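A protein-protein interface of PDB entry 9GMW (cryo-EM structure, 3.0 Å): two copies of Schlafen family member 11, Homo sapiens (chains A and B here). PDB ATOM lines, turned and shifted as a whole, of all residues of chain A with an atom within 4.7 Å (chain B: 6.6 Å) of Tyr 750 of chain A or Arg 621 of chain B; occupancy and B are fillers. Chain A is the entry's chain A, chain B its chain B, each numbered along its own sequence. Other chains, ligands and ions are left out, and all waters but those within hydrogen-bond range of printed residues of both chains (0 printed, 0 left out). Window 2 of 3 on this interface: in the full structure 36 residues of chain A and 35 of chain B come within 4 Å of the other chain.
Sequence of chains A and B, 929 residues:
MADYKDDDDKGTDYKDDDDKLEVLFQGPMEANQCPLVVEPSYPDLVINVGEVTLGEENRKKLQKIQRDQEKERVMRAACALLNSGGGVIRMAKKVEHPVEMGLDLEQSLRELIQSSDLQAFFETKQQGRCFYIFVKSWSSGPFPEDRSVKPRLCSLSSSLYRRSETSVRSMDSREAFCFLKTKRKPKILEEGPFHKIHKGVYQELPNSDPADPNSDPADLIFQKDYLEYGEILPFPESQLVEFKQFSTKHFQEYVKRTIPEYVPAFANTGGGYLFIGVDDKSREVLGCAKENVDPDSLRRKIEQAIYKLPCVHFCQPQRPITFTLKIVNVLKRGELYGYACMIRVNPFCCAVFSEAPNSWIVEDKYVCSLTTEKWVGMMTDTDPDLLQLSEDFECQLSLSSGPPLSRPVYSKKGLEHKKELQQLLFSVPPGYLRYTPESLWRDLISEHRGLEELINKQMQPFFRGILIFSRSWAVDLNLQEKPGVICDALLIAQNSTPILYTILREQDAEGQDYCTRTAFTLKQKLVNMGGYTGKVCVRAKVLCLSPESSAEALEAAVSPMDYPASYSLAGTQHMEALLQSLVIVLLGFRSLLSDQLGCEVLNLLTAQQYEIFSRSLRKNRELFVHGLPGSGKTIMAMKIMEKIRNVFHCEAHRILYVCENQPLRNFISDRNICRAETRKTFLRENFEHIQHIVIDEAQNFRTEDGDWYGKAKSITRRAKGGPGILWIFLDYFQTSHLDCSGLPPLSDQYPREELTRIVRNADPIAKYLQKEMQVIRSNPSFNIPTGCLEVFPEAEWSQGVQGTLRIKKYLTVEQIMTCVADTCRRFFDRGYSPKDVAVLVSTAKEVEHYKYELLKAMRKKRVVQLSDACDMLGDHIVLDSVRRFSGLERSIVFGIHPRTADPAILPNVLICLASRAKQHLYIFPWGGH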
ATOM      1  N   PHE A 624     -18.512 -20.625  -2.329  1.00  0.00           N
ATOM      2  CA  PHE A 624     -17.993 -19.335  -1.897  1.00  0.00           C
ATOM      3  C   PHE A 624     -18.531 -19.050  -0.504  1.00  0.00           C
ATOM      4  O   PHE A 624     -19.747 -18.977  -0.309  1.00  0.00           O
ATOM      5  CB  PHE A 624     -18.398 -18.226  -2.866  1.00  0.00           C
ATOM      6  CG  PHE A 624     -17.794 -18.367  -4.229  1.00  0.00           C
ATOM      7  CD1 PHE A 624     -18.335 -19.243  -5.151  1.00  0.00           C
ATOM      8  CD2 PHE A 624     -16.686 -17.626  -4.589  1.00  0.00           C
ATOM      9  CE1 PHE A 624     -17.781 -19.377  -6.403  1.00  0.00           C
ATOM     10  CE2 PHE A 624     -16.129 -17.758  -5.840  1.00  0.00           C
ATOM     11  CZ  PHE A 624     -16.678 -18.632  -6.747  1.00  0.00           C
ATOM     12  N   LEU A 746     -19.970 -11.074  -8.618  1.00  0.00           N
ATOM     13  CA  LEU A 746     -20.834 -11.453  -7.506  1.00  0.00           C
ATOM     14  C   LEU A 746     -21.964 -12.361  -7.971  1.00  0.00           C
ATOM     15  O   LEU A 746     -22.307 -13.327  -7.280  1.00  0.00           O
ATOM     16  CB  LEU A 746     -21.397 -10.200  -6.833  1.00  0.00           C
ATOM     17  CG  LEU A 746     -22.393 -10.425  -5.693  1.00  0.00           C
ATOM     18  CD1 LEU A 746     -21.737 -11.172  -4.545  1.00  0.00           C
ATOM     19  CD2 LEU A 746     -22.960  -9.099  -5.215  1.00  0.00           C
ATOM     20  N   SER A 747     -22.544 -12.077  -9.137  1.00  0.00           N
ATOM     21  CA  SER A 747     -23.622 -12.907  -9.656  1.00  0.00           C
ATOM     22  C   SER A 747     -23.170 -14.334  -9.935  1.00  0.00           C
ATOM     23  O   SER A 747     -24.006 -15.243  -9.938  1.00  0.00           O
ATOM     24  CB  SER A 747     -24.182 -12.286 -10.934  1.00  0.00           C
ATOM     25  OG  SER A 747     -23.151 -12.048 -11.877  1.00  0.00           O
ATOM     26  N   ASP A 748     -21.876 -14.552 -10.162  1.00  0.00           N
ATOM     27  CA  ASP A 748     -21.355 -15.869 -10.498  1.00  0.00           C
ATOM     28  C   ASP A 748     -20.763 -16.611  -9.310  1.00  0.00           C
ATOM     29  O   ASP A 748     -20.294 -17.742  -9.480  1.00  0.00           O
ATOM     30  CB  ASP A 748     -20.286 -15.744 -11.594  1.00  0.00           C
ATOM     31  CG  ASP A 748     -20.016 -17.057 -12.298  1.00  0.00           C
ATOM     32  OD1 ASP A 748     -20.959 -17.862 -12.441  1.00  0.00           O
ATOM     33  OD2 ASP A 748     -18.861 -17.284 -12.711  1.00  0.00           O
ATOM     34  N   GLN A 749     -20.769 -16.015  -8.118  1.00  0.00           N
ATOM     35  CA  GLN A 749     -20.202 -16.660  -6.939  1.00  0.00           C
ATOM     36  C   GLN A 749     -21.227 -17.549  -6.248  1.00  0.00           C
ATOM     37  O   GLN A 749     -21.710 -17.213  -5.162  1.00  0.00           O
ATOM     38  CB  GLN A 749     -19.676 -15.607  -5.963  1.00  0.00           C
ATOM     39  CG  GLN A 749     -18.385 -14.938  -6.409  1.00  0.00           C
ATOM     40  CD  GLN A 749     -18.093 -13.663  -5.645  1.00  0.00           C
ATOM     41  OE1 GLN A 749     -18.837 -13.283  -4.741  1.00  0.00           O
ATOM     42  NE2 GLN A 749     -17.000 -13.000  -5.999  1.00  0.00           N
ATOM     43  N   TYR A 750     -21.563 -18.678  -6.865  1.00  0.00           N
ATOM     44  CA  TYR A 750     -22.532 -19.620  -6.324  1.00  0.00           C
ATOM     45  C   TYR A 750     -22.034 -21.041  -6.537  1.00  0.00           C
ATOM     46  O   TYR A 750     -21.309 -21.306  -7.503  1.00  0.00           O
ATOM     47  CB  TYR A 750     -23.906 -19.458  -6.985  1.00  0.00           C
ATOM     48  CG  TYR A 750     -24.688 -18.290  -6.451  1.00  0.00           C
ATOM     49  CD1 TYR A 750     -25.386 -18.388  -5.260  1.00  0.00           C
ATOM     50  CD2 TYR A 750     -24.716 -17.083  -7.128  1.00  0.00           C
ATOM     51  CE1 TYR A 750     -26.100 -17.322  -4.764  1.00  0.00           C
ATOM     52  CE2 TYR A 750     -25.423 -16.010  -6.640  1.00  0.00           C
ATOM     53  CZ  TYR A 750     -26.114 -16.135  -5.457  1.00  0.00           C
ATOM     54  OH  TYR A 750     -26.823 -15.066  -4.965  1.00  0.00           O
ATOM     55  N   PRO A 751     -22.409 -21.981  -5.656  1.00  0.00           N
ATOM     56  CA  PRO A 751     -23.256 -21.833  -4.464  1.00  0.00           C
ATOM     57  C   PRO A 751     -22.576 -20.993  -3.396  1.00  0.00           C
ATOM     58  O   PRO A 751     -21.359 -20.847  -3.405  1.00  0.00           O
ATOM     59  CB  PRO A 751     -23.468 -23.282  -4.013  1.00  0.00           C
ATOM     60  CG  PRO A 751     -22.248 -23.995  -4.473  1.00  0.00           C
ATOM     61  CD  PRO A 751     -21.906 -23.357  -5.792  1.00  0.00           C
ATOM     62  N   ARG A 752     -23.333 -20.422  -2.466  1.00  0.00           N
ATOM     63  CA  ARG A 752     -22.798 -19.448  -1.530  1.00  0.00           C
ATOM     64  C   ARG A 752     -23.188 -19.807  -0.107  1.00  0.00           C
ATOM     65  O   ARG A 752     -24.336 -20.167   0.161  1.00  0.00           O
ATOM     66  CB  ARG A 752     -23.302 -18.046  -1.866  1.00  0.00           C
ATOM     67  CG  ARG A 752     -22.801 -16.980  -0.932  1.00  0.00           C
ATOM     68  CD  ARG A 752     -22.357 -15.765  -1.700  1.00  0.00           C
ATOM     69  NE  ARG A 752     -23.487 -15.036  -2.263  1.00  0.00           N
ATOM     70  CZ  ARG A 752     -23.532 -14.536  -3.491  1.00  0.00           C
ATOM     71  NH1 ARG A 752     -22.530 -14.689  -4.342  1.00  0.00           N
ATOM     72  NH2 ARG A 752     -24.614 -13.867  -3.878  1.00  0.00           N
ATOM     73  N   SER B 616     -32.234 -23.190   1.071  1.00  0.00           N
ATOM     74  CA  SER B 616     -31.255 -23.331   0.001  1.00  0.00           C
ATOM     75  C   SER B 616     -31.526 -22.406  -1.176  1.00  0.00           C
ATOM     76  O   SER B 616     -30.701 -22.349  -2.093  1.00  0.00           O
ATOM     77  CB  SER B 616     -31.223 -24.776  -0.494  1.00  0.00           C
ATOM     78  OG  SER B 616     -30.711 -25.645   0.500  1.00  0.00           O
ATOM     79  N   LEU B 617     -32.651 -21.691  -1.187  1.00  0.00           N
ATOM     80  CA  LEU B 617     -32.936 -20.799  -2.304  1.00  0.00           C
ATOM     81  C   LEU B 617     -31.976 -19.617  -2.335  1.00  0.00           C
ATOM     82  O   LEU B 617     -31.636 -19.123  -3.416  1.00  0.00           O
ATOM     83  CB  LEU B 617     -34.379 -20.305  -2.230  1.00  0.00           C
ATOM     84  CG  LEU B 617     -34.869 -19.519  -3.447  1.00  0.00           C
ATOM     85  CD1 LEU B 617     -34.753 -20.354  -4.708  1.00  0.00           C
ATOM     86  CD2 LEU B 617     -36.298 -19.044  -3.247  1.00  0.00           C
ATOM     87  N   ARG B 618     -31.538 -19.145  -1.167  1.00  0.00           N
ATOM     88  CA  ARG B 618     -30.583 -18.047  -1.109  1.00  0.00           C
ATOM     89  C   ARG B 618     -29.158 -18.505  -1.392  1.00  0.00           C
ATOM     90  O   ARG B 618     -28.294 -17.669  -1.666  1.00  0.00           O
ATOM     91  CB  ARG B 618     -30.646 -17.384   0.268  1.00  0.00           C
ATOM     92  CG  ARG B 618     -29.922 -16.050   0.369  1.00  0.00           C
ATOM     93  CD  ARG B 618     -29.206 -15.902   1.709  1.00  0.00           C
ATOM     94  NE  ARG B 618     -29.427 -14.597   2.321  1.00  0.00           N
ATOM     95  CZ  ARG B 618     -28.788 -13.487   1.975  1.00  0.00           C
ATOM     96  NH1 ARG B 618     -27.882 -13.482   1.011  1.00  0.00           N
ATOM     97  NH2 ARG B 618     -29.065 -12.355   2.614  1.00  0.00           N
ATOM     98  N   LYS B 619     -28.899 -19.811  -1.349  1.00  0.00           N
ATOM     99  CA  LYS B 619     -27.544 -20.333  -1.395  1.00  0.00           C
ATOM    100  C   LYS B 619     -27.207 -21.069  -2.683  1.00  0.00           C
ATOM    101  O   LYS B 619     -26.073 -21.541  -2.820  1.00  0.00           O
ATOM    102  CB  LYS B 619     -27.312 -21.279  -0.211  1.00  0.00           C
ATOM    103  CG  LYS B 619     -27.533 -20.629   1.145  1.00  0.00           C
ATOM    104  CD  LYS B 619     -28.240 -21.558   2.123  1.00  0.00           C
ATOM    105  CE  LYS B 619     -27.295 -22.581   2.724  1.00  0.00           C
ATOM    106  NZ  LYS B 619     -26.667 -23.461   1.704  1.00  0.00           N
ATOM    107  N   ASN B 620     -28.143 -21.190  -3.622  1.00  0.00           N
ATOM    108  CA  ASN B 620     -27.894 -21.920  -4.855  1.00  0.00           C
ATOM    109  C   ASN B 620     -28.641 -21.264  -6.006  1.00  0.00           C
ATOM    110  O   ASN B 620     -29.648 -20.580  -5.814  1.00  0.00           O
ATOM    111  CB  ASN B 620     -28.322 -23.389  -4.742  1.00  0.00           C
ATOM    112  CG  ASN B 620     -27.613 -24.121  -3.625  1.00  0.00           C
ATOM    113  OD1 ASN B 620     -26.532 -24.670  -3.817  1.00  0.00           O
ATOM    114  ND2 ASN B 620     -28.223 -24.138  -2.449  1.00  0.00           N
ATOM    115  N   ARG B 621     -28.118 -21.475  -7.214  1.00  0.00           N
ATOM    116  CA  ARG B 621     -28.841 -21.152  -8.437  1.00  0.00           C
ATOM    117  C   ARG B 621     -29.088 -22.437  -9.216  1.00  0.00           C
ATOM    118  O   ARG B 621     -30.229 -22.747  -9.571  1.00  0.00           O
ATOM    119  CB  ARG B 621     -28.062 -20.139  -9.279  1.00  0.00           C
ATOM    120  CG  ARG B 621     -27.953 -18.766  -8.646  1.00  0.00           C
ATOM    121  CD  ARG B 621     -29.299 -18.071  -8.575  1.00  0.00           C
ATOM    122  NE  ARG B 621     -29.259 -16.884  -7.729  1.00  0.00           N
ATOM    123  CZ  ARG B 621     -29.705 -16.829  -6.481  1.00  0.00           C
ATOM    124  NH1 ARG B 621     -30.203 -17.895  -5.872  1.00  0.00           N
ATOM    125  NH2 ARG B 621     -29.642 -15.677  -5.820  1.00  0.00           N
ATOM    126  N   GLU B 622     -28.023 -23.186  -9.485  1.00  0.00           N
ATOM    127  CA  GLU B 622     -28.168 -24.559  -9.942  1.00  0.00           C
ATOM    128  C   GLU B 622     -28.230 -25.485  -8.735  1.00  0.00           C
ATOM    129  O   GLU B 622     -27.425 -25.371  -7.810  1.00  0.00           O
ATOM    130  CB  GLU B 622     -26.995 -24.955 -10.840  1.00  0.00           C
ATOM    131  CG  GLU B 622     -27.173 -24.627 -12.313  1.00  0.00           C
ATOM    132  CD  GLU B 622     -27.424 -23.155 -12.568  1.00  0.00           C
ATOM    133  OE1 GLU B 622     -27.501 -22.760 -13.750  1.00  0.00           O
ATOM    134  OE2 GLU B 622     -27.546 -22.389 -11.589  1.00  0.00           O
ATOM    135  N   LEU B 623     -29.194 -26.400  -8.739  1.00  0.00           N
ATOM    136  CA  LEU B 623     -29.344 -27.328  -7.628  1.00  0.00           C
ATOM    137  C   LEU B 623     -29.962 -28.619  -8.137  1.00  0.00           C
ATOM    138  O   LEU B 623     -30.944 -28.587  -8.882  1.00  0.00           O
ATOM    139  CB  LEU B 623     -30.206 -26.717  -6.518  1.00  0.00           C
ATOM    140  CG  LEU B 623     -30.332 -27.516  -5.220  1.00  0.00           C
ATOM    141  CD1 LEU B 623     -28.978 -27.800  -4.612  1.00  0.00           C
ATOM    142  CD2 LEU B 623     -31.199 -26.769  -4.233  1.00  0.00           C
ATOM    143  N   PHE B 648     -38.163 -13.069  -5.693  1.00  0.00           N
ATOM    144  CA  PHE B 648     -37.701 -12.314  -6.846  1.00  0.00           C
ATOM    145  C   PHE B 648     -38.770 -11.401  -7.432  1.00  0.00           C
ATOM    146  O   PHE B 648     -38.473 -10.657  -8.372  1.00  0.00           O
ATOM    147  CB  PHE B 648     -37.190 -13.263  -7.939  1.00  0.00           C
ATOM    148  CG  PHE B 648     -36.066 -14.165  -7.495  1.00  0.00           C
ATOM    149  CD1 PHE B 648     -36.257 -15.115  -6.505  1.00  0.00           C
ATOM    150  CD2 PHE B 648     -34.815 -14.060  -8.074  1.00  0.00           C
ATOM    151  CE1 PHE B 648     -35.226 -15.941  -6.105  1.00  0.00           C
ATOM    152  CE2 PHE B 648     -33.780 -14.884  -7.676  1.00  0.00           C
ATOM    153  CZ  PHE B 648     -33.987 -15.825  -6.690  1.00  0.00           C
ATOM    154  N   ILE B 693     -36.330 -21.687 -14.013  1.00  0.00           N
ATOM    155  CA  ILE B 693     -36.771 -22.975 -14.532  1.00  0.00           C
ATOM    156  C   ILE B 693     -36.688 -24.003 -13.415  1.00  0.00           C
ATOM    157  O   ILE B 693     -35.664 -24.099 -12.730  1.00  0.00           O
ATOM    158  CB  ILE B 693     -35.925 -23.414 -15.741  1.00  0.00           C
ATOM    159  CG1 ILE B 693     -36.194 -22.484 -16.927  1.00  0.00           C
ATOM    160  CG2 ILE B 693     -36.213 -24.874 -16.096  1.00  0.00           C
ATOM    161  CD1 ILE B 693     -35.464 -22.860 -18.195  1.00  0.00           C
ATOM    162  N   GLY B 721     -30.932 -10.175 -13.967  1.00  0.00           N
ATOM    163  CA  GLY B 721     -30.429 -10.063 -12.614  1.00  0.00           C
ATOM    164  C   GLY B 721     -29.531 -11.222 -12.240  1.00  0.00           C
ATOM    165  O   GLY B 721     -29.747 -11.882 -11.218  1.00  0.00           O
ATOM    166  N   GLY B 722     -28.515 -11.478 -13.059  1.00  0.00           N
ATOM    167  CA  GLY B 722     -27.655 -12.618 -12.869  1.00  0.00           C
ATOM    168  C   GLY B 722     -28.335 -13.880 -13.352  1.00  0.00           C
ATOM    169  O   GLY B 722     -29.487 -13.856 -13.794  1.00  0.00           O
ATOM    170  N   PRO B 723     -27.638 -15.012 -13.277  1.00  0.00           N
ATOM    171  CA  PRO B 723     -28.257 -16.275 -13.692  1.00  0.00           C
ATOM    172  C   PRO B 723     -29.495 -16.580 -12.863  1.00  0.00           C
ATOM    173  O   PRO B 723     -29.547 -16.304 -11.663  1.00  0.00           O
ATOM    174  CB  PRO B 723     -27.147 -17.308 -13.462  1.00  0.00           C
ATOM    175  CG  PRO B 723     -26.237 -16.682 -12.465  1.00  0.00           C
ATOM    176  CD  PRO B 723     -26.288 -15.209 -12.724  1.00  0.00           C
ATOM    177  N   GLY B 724     -30.500 -17.147 -13.518  1.00  0.00           N
ATOM    178  CA  GLY B 724     -31.732 -17.485 -12.842  1.00  0.00           C
ATOM    179  C   GLY B 724     -31.665 -18.835 -12.154  1.00  0.00           C
ATOM    180  O   GLY B 724     -30.685 -19.576 -12.233  1.00  0.00           O
ATOM    181  N   ILE B 725     -32.754 -19.155 -11.457  1.00  0.00           N
ATOM    182  CA  ILE B 725     -32.859 -20.426 -10.755  1.00  0.00           C
ATOM    183  C   ILE B 725     -32.981 -21.554 -11.769  1.00  0.00           C
ATOM    184  O   ILE B 725     -33.752 -21.464 -12.732  1.00  0.00           O
ATOM    185  CB  ILE B 725     -34.064 -20.412  -9.804  1.00  0.00           C
ATOM    186  CG1 ILE B 725     -33.907 -19.330  -8.732  1.00  0.00           C
ATOM    187  CG2 ILE B 725     -34.241 -21.771  -9.160  1.00  0.00           C
ATOM    188  CD1 ILE B 725     -32.807 -19.595  -7.733  1.00  0.00           C
ATOM    189  N   LEU B 726     -32.216 -22.624 -11.561  1.00  0.00           N
ATOM    190  CA  LEU B 726     -32.338 -23.851 -12.346  1.00  0.00           C
ATOM    191  C   LEU B 726     -32.227 -25.023 -11.378  1.00  0.00           C
ATOM    192  O   LEU B 726     -31.131 -25.527 -11.131  1.00  0.00           O
ATOM    193  CB  LEU B 726     -31.277 -23.928 -13.436  1.00  0.00           C
ATOM    194  CG  LEU B 726     -31.289 -25.222 -14.254  1.00  0.00           C
ATOM    195  CD1 LEU B 726     -32.644 -25.429 -14.905  1.00  0.00           C
ATOM    196  CD2 LEU B 726     -30.196 -25.213 -15.300  1.00  0.00           C
ATOM    197  N   TRP B 727     -33.364 -25.463 -10.846  1.00  0.00           N
ATOM    198  CA  TRP B 727     -33.414 -26.581  -9.916  1.00  0.00           C
ATOM    199  C   TRP B 727     -33.993 -27.794 -10.625  1.00  0.00           C
ATOM    200  O   TRP B 727     -35.034 -27.694 -11.283  1.00  0.00           O
ATOM    201  CB  TRP B 727     -34.246 -26.229  -8.683  1.00  0.00           C
ATOM    202  CG  TRP B 727     -33.540 -25.303  -7.738  1.00  0.00           C
ATOM    203  CD1 TRP B 727     -32.508 -24.465  -8.036  1.00  0.00           C
ATOM    204  CD2 TRP B 727     -33.810 -25.124  -6.345  1.00  0.00           C
ATOM    205  NE1 TRP B 727     -32.121 -23.772  -6.919  1.00  0.00           N
ATOM    206  CE2 TRP B 727     -32.904 -24.160  -5.865  1.00  0.00           C
ATOM    207  CE3 TRP B 727     -34.729 -25.686  -5.455  1.00  0.00           C
ATOM    208  CZ2 TRP B 727     -32.892 -23.745  -4.538  1.00  0.00           C
ATOM    209  CZ3 TRP B 727     -34.714 -25.271  -4.140  1.00  0.00           C
ATOM    210  CH2 TRP B 727     -33.802 -24.312  -3.693  1.00  0.00           C
ATOM    211  N   PRO B 751     -24.439 -28.145  -7.144  1.00  0.00           N
ATOM    212  CA  PRO B 751     -24.644 -28.568  -5.752  1.00  0.00           C
ATOM    213  C   PRO B 751     -25.871 -29.460  -5.606  1.00  0.00           C
ATOM    214  O   PRO B 751     -26.710 -29.512  -6.498  1.00  0.00           O
ATOM    215  CB  PRO B 751     -24.799 -27.236  -5.013  1.00  0.00           C
ATOM    216  CG  PRO B 751     -25.388 -26.321  -6.023  1.00  0.00           C
ATOM    217  CD  PRO B 751     -24.765 -26.722  -7.330  1.00  0.00           C
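Printed residues of chain B that touch a printed residue of chain A: Arg 618, Lys 619, Asn 620, Arg 621, Gly 722 and Pro 723.
Of the 8 printed residues of chain A, 4 touch a printed residue of chain B.
Among the printed residues, 7 pairs touch across the chains.
Among the printed residues, merely in contact across the chains: Pro 751 of chain A with Lys 619 of chain B, Pro 751 of chain A with Asn 620 of chain B, Ser 747 of chain A with Pro 723 of chain B, Tyr 750 of chain A with Arg 618 of chain B and Ser 747 of chain A with Gly 722 of chain B.
Position printed for both chains: 751.
Tyr 750 of chain A touches two residues of chain B.
Of the printed residues of chain A, Arg 618 of chain B touches Tyr 750.
Of the printed residues of chain A, Lys 619 of chain B touches Pro 751 (3.3 Å) and Arg 752 (3.0 Å).
Printed residues of chain A within 4 Å of Pro 723 of chain B: Ser 747 (3.6 Å).
The nearest printed residue of chain A that does not touch Asn 620 of chain B is Tyr 750 of chain A (4.3 Å).
OH of Tyr 750 of chain A is in hydrogen-bond range of NH2 of Arg 621 of chain B.
O of Lys 619 of chain B sits at hydrogen-bond distance from N of Arg 752 of chain A (3.0 Å).
N of Leu 726 of chain B sits at hydrogen-bond distance from O of Arg 621 of chain B, at 2.8 Å.
NH1 of Arg 752 of chain A lies within hydrogen-bond range of O of Leu 746 of chain A, 3.2 Å away.
The backbone carbonyl oxygen of Gln 749 of chain A sits at hydrogen-bond distance from the guanidinium group of Arg 752 of chain A (2.8 Å).
OH of Tyr 750 of chain A lies within hydrogen-bond range of NH2 of Arg 752 of chain A, 2.7 Å away.
The backbone carbonyl oxygen (O) of Leu 617 of chain B is in hydrogen-bond range of the guanidinium group (NH1) of Arg 621 of chain B (3.1 Å).
The indole nitrogen (NE1) of Trp 727 of chain B lies close to the backbone carbonyl oxygen (O) of Arg 621 of chain B, at 3.4 Å.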
